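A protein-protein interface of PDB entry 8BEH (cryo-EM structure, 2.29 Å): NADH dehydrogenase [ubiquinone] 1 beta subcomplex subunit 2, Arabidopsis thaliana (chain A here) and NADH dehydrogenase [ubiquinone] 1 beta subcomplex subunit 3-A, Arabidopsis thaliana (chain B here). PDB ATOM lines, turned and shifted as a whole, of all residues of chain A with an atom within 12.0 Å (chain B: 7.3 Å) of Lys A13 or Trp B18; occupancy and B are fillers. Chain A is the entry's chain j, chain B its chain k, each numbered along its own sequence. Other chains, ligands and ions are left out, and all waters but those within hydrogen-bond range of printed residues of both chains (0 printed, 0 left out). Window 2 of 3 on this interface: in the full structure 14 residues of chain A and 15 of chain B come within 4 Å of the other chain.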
ATOM      1  N   GLY A   9     -41.091   4.861  15.685  1.00  0.00           N
ATOM      2  CA  GLY A   9     -40.144   4.606  14.616  1.00  0.00           C
ATOM      3  C   GLY A   9     -39.535   3.215  14.614  1.00  0.00           C
ATOM      4  O   GLY A   9     -39.637   2.477  15.594  1.00  0.00           O
ATOM      5  N   ILE A  10     -38.896   2.860  13.500  1.00  0.00           N
ATOM      6  CA  ILE A  10     -38.246   1.566  13.328  1.00  0.00           C
ATOM      7  C   ILE A  10     -36.741   1.779  13.261  1.00  0.00           C
ATOM      8  O   ILE A  10     -36.257   2.613  12.486  1.00  0.00           O
ATOM      9  CB  ILE A  10     -38.761   0.851  12.067  1.00  0.00           C
ATOM     10  CG1 ILE A  10     -40.286   0.731  12.119  1.00  0.00           C
ATOM     11  CG2 ILE A  10     -38.129  -0.526  11.934  1.00  0.00           C
ATOM     12  CD1 ILE A  10     -40.981   1.269  10.897  1.00  0.00           C
ATOM     13  N   THR A  11     -36.000   1.029  14.072  1.00  0.00           N
ATOM     14  CA  THR A  11     -34.558   1.199  14.211  1.00  0.00           C
ATOM     15  C   THR A  11     -33.850   0.051  13.506  1.00  0.00           C
ATOM     16  O   THR A  11     -34.073  -1.118  13.837  1.00  0.00           O
ATOM     17  CB  THR A  11     -34.154   1.255  15.681  1.00  0.00           C
ATOM     18  OG1 THR A  11     -34.796   2.370  16.312  1.00  0.00           O
ATOM     19  CG2 THR A  11     -32.649   1.412  15.811  1.00  0.00           C
ATOM     20  N   TYR A  12     -32.994   0.386  12.543  1.00  0.00           N
ATOM     21  CA  TYR A  12     -32.222  -0.593  11.785  1.00  0.00           C
ATOM     22  C   TYR A  12     -30.747  -0.235  11.892  1.00  0.00           C
ATOM     23  O   TYR A  12     -30.304   0.759  11.304  1.00  0.00           O
ATOM     24  CB  TYR A  12     -32.661  -0.633  10.323  1.00  0.00           C
ATOM     25  CG  TYR A  12     -32.210  -1.863   9.578  1.00  0.00           C
ATOM     26  CD1 TYR A  12     -31.641  -2.936  10.245  1.00  0.00           C
ATOM     27  CD2 TYR A  12     -32.310  -1.931   8.199  1.00  0.00           C
ATOM     28  CE1 TYR A  12     -31.218  -4.056   9.562  1.00  0.00           C
ATOM     29  CE2 TYR A  12     -31.887  -3.042   7.506  1.00  0.00           C
ATOM     30  CZ  TYR A  12     -31.343  -4.103   8.191  1.00  0.00           C
ATOM     31  OH  TYR A  12     -30.920  -5.213   7.499  1.00  0.00           O
ATOM     32  N   LYS A  13     -29.995  -1.058  12.628  1.00  0.00           N
ATOM     33  CA  LYS A  13     -28.562  -0.903  12.872  1.00  0.00           C
ATOM     34  C   LYS A  13     -28.145   0.549  13.080  1.00  0.00           C
ATOM     35  O   LYS A  13     -27.366   1.102  12.296  1.00  0.00           O
ATOM     36  CB  LYS A  13     -27.722  -1.560  11.763  1.00  0.00           C
ATOM     37  CG  LYS A  13     -28.094  -1.286  10.320  1.00  0.00           C
ATOM     38  CD  LYS A  13     -27.089  -1.947   9.394  1.00  0.00           C
ATOM     39  CE  LYS A  13     -27.573  -3.275   8.838  1.00  0.00           C
ATOM     40  NZ  LYS A  13     -28.518  -3.110   7.703  1.00  0.00           N
ATOM     41  N   GLY A  14     -28.647   1.161  14.135  1.00  0.00           N
ATOM     42  CA  GLY A  14     -28.266   2.519  14.501  1.00  0.00           C
ATOM     43  C   GLY A  14     -29.185   3.615  14.035  1.00  0.00           C
ATOM     44  O   GLY A  14     -29.552   4.493  14.814  1.00  0.00           O
ATOM     45  N   VAL A  15     -29.562   3.587  12.766  1.00  0.00           N
ATOM     46  CA  VAL A  15     -30.392   4.640  12.198  1.00  0.00           C
ATOM     47  C   VAL A  15     -31.855   4.362  12.516  1.00  0.00           C
ATOM     48  O   VAL A  15     -32.362   3.262  12.275  1.00  0.00           O
ATOM     49  CB  VAL A  15     -30.153   4.755  10.686  1.00  0.00           C
ATOM     50  CG1 VAL A  15     -31.114   5.741  10.078  1.00  0.00           C
ATOM     51  CG2 VAL A  15     -28.712   5.171  10.420  1.00  0.00           C
ATOM     52  N   THR A  16     -32.535   5.364  13.060  1.00  0.00           N
ATOM     53  CA  THR A  16     -33.942   5.271  13.418  1.00  0.00           C
ATOM     54  C   THR A  16     -34.749   6.199  12.524  1.00  0.00           C
ATOM     55  O   THR A  16     -34.444   7.391  12.424  1.00  0.00           O
ATOM     56  CB  THR A  16     -34.155   5.634  14.889  1.00  0.00           C
ATOM     57  OG1 THR A  16     -33.858   4.496  15.708  1.00  0.00           O
ATOM     58  CG2 THR A  16     -35.589   6.061  15.136  1.00  0.00           C
ATOM     59  N   VAL A  17     -35.773   5.655  11.876  1.00  0.00           N
ATOM     60  CA  VAL A  17     -36.642   6.426  10.996  1.00  0.00           C
ATOM     61  C   VAL A  17     -38.024   6.483  11.628  1.00  0.00           C
ATOM     62  O   VAL A  17     -38.603   5.443  11.965  1.00  0.00           O
ATOM     63  CB  VAL A  17     -36.700   5.824   9.582  1.00  0.00           C
ATOM     64  CG1 VAL A  17     -37.274   6.836   8.600  1.00  0.00           C
ATOM     65  CG2 VAL A  17     -35.325   5.373   9.142  1.00  0.00           C
ATOM     66  N   HIS A  18     -38.538   7.694  11.808  1.00  0.00           N
ATOM     67  CA  HIS A  18     -39.846   7.905  12.406  1.00  0.00           C
ATOM     68  C   HIS A  18     -40.938   7.813  11.353  1.00  0.00           C
ATOM     69  O   HIS A  18     -40.817   8.377  10.263  1.00  0.00           O
ATOM     70  CB  HIS A  18     -39.921   9.265  13.101  1.00  0.00           C
ATOM     71  CG  HIS A  18     -38.685   9.632  13.859  1.00  0.00           C
ATOM     72  ND1 HIS A  18     -38.474   9.243  15.163  1.00  0.00           N
ATOM     73  CD2 HIS A  18     -37.603  10.365  13.506  1.00  0.00           C
ATOM     74  CE1 HIS A  18     -37.312   9.712  15.578  1.00  0.00           C
ATOM     75  NE2 HIS A  18     -36.762  10.396  14.590  1.00  0.00           N
ATOM     76  N   ARG B  13     -18.931   0.171   1.385  1.00  0.00           N
ATOM     77  CA  ARG B  13     -20.197  -0.544   1.258  1.00  0.00           C
ATOM     78  C   ARG B  13     -20.614  -1.171   2.582  1.00  0.00           C
ATOM     79  O   ARG B  13     -21.803  -1.182   2.921  1.00  0.00           O
ATOM     80  CB  ARG B  13     -20.096  -1.613   0.175  1.00  0.00           C
ATOM     81  CG  ARG B  13     -21.414  -2.293  -0.108  1.00  0.00           C
ATOM     82  CD  ARG B  13     -21.252  -3.432  -1.096  1.00  0.00           C
ATOM     83  NE  ARG B  13     -20.608  -4.639  -0.573  1.00  0.00           N
ATOM     84  CZ  ARG B  13     -20.804  -5.200   0.618  1.00  0.00           C
ATOM     85  NH1 ARG B  13     -21.717  -4.753   1.466  1.00  0.00           N
ATOM     86  NH2 ARG B  13     -20.089  -6.271   0.951  1.00  0.00           N
ATOM     87  N   ARG B  14     -19.652  -1.696   3.343  1.00  0.00           N
ATOM     88  CA  ARG B  14     -19.966  -2.237   4.659  1.00  0.00           C
ATOM     89  C   ARG B  14     -20.539  -1.165   5.573  1.00  0.00           C
ATOM     90  O   ARG B  14     -21.489  -1.421   6.320  1.00  0.00           O
ATOM     91  CB  ARG B  14     -18.717  -2.856   5.282  1.00  0.00           C
ATOM     92  CG  ARG B  14     -18.536  -4.315   4.959  1.00  0.00           C
ATOM     93  CD  ARG B  14     -17.628  -4.996   5.952  1.00  0.00           C
ATOM     94  NE  ARG B  14     -16.783  -5.999   5.320  1.00  0.00           N
ATOM     95  CZ  ARG B  14     -15.591  -6.364   5.766  1.00  0.00           C
ATOM     96  NH1 ARG B  14     -15.066  -5.827   6.854  1.00  0.00           N
ATOM     97  NH2 ARG B  14     -14.912  -7.298   5.108  1.00  0.00           N
ATOM     98  N   ARG B  15     -19.971   0.044   5.535  1.00  0.00           N
ATOM     99  CA  ARG B  15     -20.496   1.117   6.373  1.00  0.00           C
ATOM    100  C   ARG B  15     -21.893   1.555   5.955  1.00  0.00           C
ATOM    101  O   ARG B  15     -22.627   2.102   6.784  1.00  0.00           O
ATOM    102  CB  ARG B  15     -19.554   2.323   6.353  1.00  0.00           C
ATOM    103  CG  ARG B  15     -18.159   2.043   6.889  1.00  0.00           C
ATOM    104  CD  ARG B  15     -18.160   1.701   8.365  1.00  0.00           C
ATOM    105  NE  ARG B  15     -19.007   2.596   9.142  1.00  0.00           N
ATOM    106  CZ  ARG B  15     -19.734   2.226  10.185  1.00  0.00           C
ATOM    107  NH1 ARG B  15     -19.722   0.980  10.629  1.00  0.00           N
ATOM    108  NH2 ARG B  15     -20.481   3.130  10.807  1.00  0.00           N
ATOM    109  N   ASP B  16     -22.280   1.324   4.704  1.00  0.00           N
ATOM    110  CA  ASP B  16     -23.560   1.777   4.179  1.00  0.00           C
ATOM    111  C   ASP B  16     -24.683   0.765   4.377  1.00  0.00           C
ATOM    112  O   ASP B  16     -25.724   0.885   3.725  1.00  0.00           O
ATOM    113  CB  ASP B  16     -23.436   2.104   2.686  1.00  0.00           C
ATOM    114  CG  ASP B  16     -22.860   3.485   2.428  1.00  0.00           C
ATOM    115  OD1 ASP B  16     -23.173   4.420   3.188  1.00  0.00           O
ATOM    116  OD2 ASP B  16     -22.107   3.640   1.449  1.00  0.00           O
ATOM    117  N   GLU B  17     -24.501  -0.221   5.259  1.00  0.00           N
ATOM    118  CA  GLU B  17     -25.506  -1.272   5.410  1.00  0.00           C
ATOM    119  C   GLU B  17     -26.846  -0.719   5.876  1.00  0.00           C
ATOM    120  O   GLU B  17     -27.898  -1.226   5.472  1.00  0.00           O
ATOM    121  CB  GLU B  17     -25.006  -2.338   6.381  1.00  0.00           C
ATOM    122  CG  GLU B  17     -24.166  -3.416   5.736  1.00  0.00           C
ATOM    123  CD  GLU B  17     -23.265  -4.123   6.729  1.00  0.00           C
ATOM    124  OE1 GLU B  17     -22.072  -4.325   6.420  1.00  0.00           O
ATOM    125  OE2 GLU B  17     -23.751  -4.476   7.824  1.00  0.00           O
ATOM    126  N   TRP B  18     -26.832   0.321   6.711  1.00  0.00           N
ATOM    127  CA  TRP B  18     -28.074   0.906   7.202  1.00  0.00           C
ATOM    128  C   TRP B  18     -28.921   1.496   6.083  1.00  0.00           C
ATOM    129  O   TRP B  18     -30.123   1.694   6.269  1.00  0.00           O
ATOM    130  CB  TRP B  18     -27.768   1.978   8.250  1.00  0.00           C
ATOM    131  CG  TRP B  18     -27.126   3.211   7.693  1.00  0.00           C
ATOM    132  CD1 TRP B  18     -25.793   3.463   7.594  1.00  0.00           C
ATOM    133  CD2 TRP B  18     -27.792   4.354   7.149  1.00  0.00           C
ATOM    134  NE1 TRP B  18     -25.583   4.692   7.030  1.00  0.00           N
ATOM    135  CE2 TRP B  18     -26.794   5.264   6.748  1.00  0.00           C
ATOM    136  CE3 TRP B  18     -29.134   4.699   6.963  1.00  0.00           C
ATOM    137  CZ2 TRP B  18     -27.092   6.493   6.174  1.00  0.00           C
ATOM    138  CZ3 TRP B  18     -29.428   5.920   6.395  1.00  0.00           C
ATOM    139  CH2 TRP B  18     -28.413   6.803   6.007  1.00  0.00           C
ATOM    140  N   ARG B  19     -28.325   1.773   4.925  1.00  0.00           N
ATOM    141  CA  ARG B  19     -29.072   2.319   3.801  1.00  0.00           C
ATOM    142  C   ARG B  19     -30.019   1.306   3.175  1.00  0.00           C
ATOM    143  O   ARG B  19     -30.829   1.684   2.324  1.00  0.00           O
ATOM    144  CB  ARG B  19     -28.102   2.861   2.756  1.00  0.00           C
ATOM    145  CG  ARG B  19     -27.566   4.233   3.111  1.00  0.00           C
ATOM    146  CD  ARG B  19     -26.378   4.610   2.260  1.00  0.00           C
ATOM    147  NE  ARG B  19     -25.428   5.417   3.012  1.00  0.00           N
ATOM    148  CZ  ARG B  19     -25.427   6.742   3.033  1.00  0.00           C
ATOM    149  NH1 ARG B  19     -26.340   7.443   2.381  1.00  0.00           N
ATOM    150  NH2 ARG B  19     -24.498   7.379   3.737  1.00  0.00           N
ATOM    151  N   LYS B  20     -29.938   0.038   3.570  1.00  0.00           N
ATOM    152  CA  LYS B  20     -30.946  -0.953   3.224  1.00  0.00           C
ATOM    153  C   LYS B  20     -32.140  -0.905   4.166  1.00  0.00           C
ATOM    154  O   LYS B  20     -32.889  -1.883   4.252  1.00  0.00           O
ATOM    155  CB  LYS B  20     -30.336  -2.357   3.218  1.00  0.00           C
ATOM    156  CG  LYS B  20     -29.067  -2.508   2.404  1.00  0.00           C
ATOM    157  CD  LYS B  20     -29.145  -1.769   1.080  1.00  0.00           C
ATOM    158  CE  LYS B  20     -27.977  -2.130   0.178  1.00  0.00           C
ATOM    159  NZ  LYS B  20     -28.410  -2.447  -1.212  1.00  0.00           N
ATOM    160  N   HIS B  21     -32.323   0.210   4.870  1.00  0.00           N
ATOM    161  CA  HIS B  21     -33.472   0.390   5.744  1.00  0.00           C
ATOM    162  C   HIS B  21     -34.758   0.142   4.961  1.00  0.00           C
ATOM    163  O   HIS B  21     -34.884   0.603   3.820  1.00  0.00           O
ATOM    164  CB  HIS B  21     -33.480   1.811   6.318  1.00  0.00           C
ATOM    165  CG  HIS B  21     -34.083   1.916   7.685  1.00  0.00           C
ATOM    166  ND1 HIS B  21     -35.437   1.787   7.912  1.00  0.00           N
ATOM    167  CD2 HIS B  21     -33.524   2.184   8.888  1.00  0.00           C
ATOM    168  CE1 HIS B  21     -35.681   1.943   9.201  1.00  0.00           C
ATOM    169  NE2 HIS B  21     -34.537   2.184   9.815  1.00  0.00           N
ATOM    170  N   PRO B  22     -35.723  -0.584   5.533  1.00  0.00           N
ATOM    171  CA  PRO B  22     -36.923  -0.945   4.759  1.00  0.00           C
ATOM    172  C   PRO B  22     -37.675   0.246   4.194  1.00  0.00           C
ATOM    173  O   PRO B  22     -38.067   0.218   3.021  1.00  0.00           O
ATOM    174  CB  PRO B  22     -37.770  -1.709   5.782  1.00  0.00           C
ATOM    175  CG  PRO B  22     -36.787  -2.251   6.752  1.00  0.00           C
ATOM    176  CD  PRO B  22     -35.692  -1.241   6.851  1.00  0.00           C
ATOM    177  N   LEU B  24     -36.477   3.368   3.842  1.00  0.00           N
ATOM    178  CA  LEU B  24     -35.608   4.289   3.130  1.00  0.00           C
ATOM    179  C   LEU B  24     -35.318   3.828   1.711  1.00  0.00           C
ATOM    180  O   LEU B  24     -34.729   4.588   0.935  1.00  0.00           O
ATOM    181  CB  LEU B  24     -34.283   4.458   3.887  1.00  0.00           C
ATOM    182  CG  LEU B  24     -34.317   5.285   5.171  1.00  0.00           C
ATOM    183  CD1 LEU B  24     -32.952   5.881   5.454  1.00  0.00           C
ATOM    184  CD2 LEU B  24     -35.383   6.370   5.099  1.00  0.00           C
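The backbone carbonyl oxygen of Ile A10 sits at hydrogen-bond distance from a ring nitrogen (NE2) of His B21, 3.2 Å away.
O of Glu B17 lies within hydrogen-bond range of NZ of Lys A13, at 3.0 Å.
O of Val A15 lies within hydrogen-bond range of NE2 of His B21 (3.5 Å).
O of Val A17 sits at hydrogen-bond distance from N of Ile A10, 3.0 Å away.
OH of Tyr A12 lies close to NZ of Lys A13 (3.2 Å).
CE2 of Tyr A12 touches O of Lys B20 (3.6 Å).
CD2 of His B21 touches CB of Tyr A12, 3.3 Å away.
Pro B22 touches Tyr A12 (CD to CD2, 3.7 Å).
Lys A13 touches Trp B18 (CD to N, 3.5 Å).
Trp B18 touches Val A15 (CD2 to CG2, 3.5 Å).
Val A17 touches His B21.
Of the printed residues of chain B, Tyr A12 touches Lys B20, His B21 and Pro B22.
Lys A13 touches just these residues of chain B: Glu B17 (3.0 Å) and Trp B18 (3.5 Å).
No residue of chain A comes within 4 Å of Arg B15.
No residue of chain A comes within 4 Å of Asp B16.
Glu B17 touches just one residue of chain A: Lys A13.
Trp B18 touches just these residues of chain A: Lys A13 and Val A15.
No residue of chain A comes within 4 Å of Arg B19.
His B21 touches four residues of chain A.
Of the printed residues of chain A, Pro B22 touches Tyr A12.
The nearest residue of chain A that does not touch Trp B18 is Tyr A12 (4.2 Å).
Printed residues of chain B that touch a printed residue of chain A: Glu B17, Trp B18, Lys B20, His B21 and Pro B22.
Hydrophobic or aromatic side chains of chain B that line the printed part of chain A: Trp B18, His B21 and Pro B22.
Of the 10 printed residues of chain A, 5 touch a printed residue of chain B.
Among the printed residues, no Asp or Glu carboxylate lies within 4 Å of a Lys or Arg side-chain nitrogen of the other chain.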
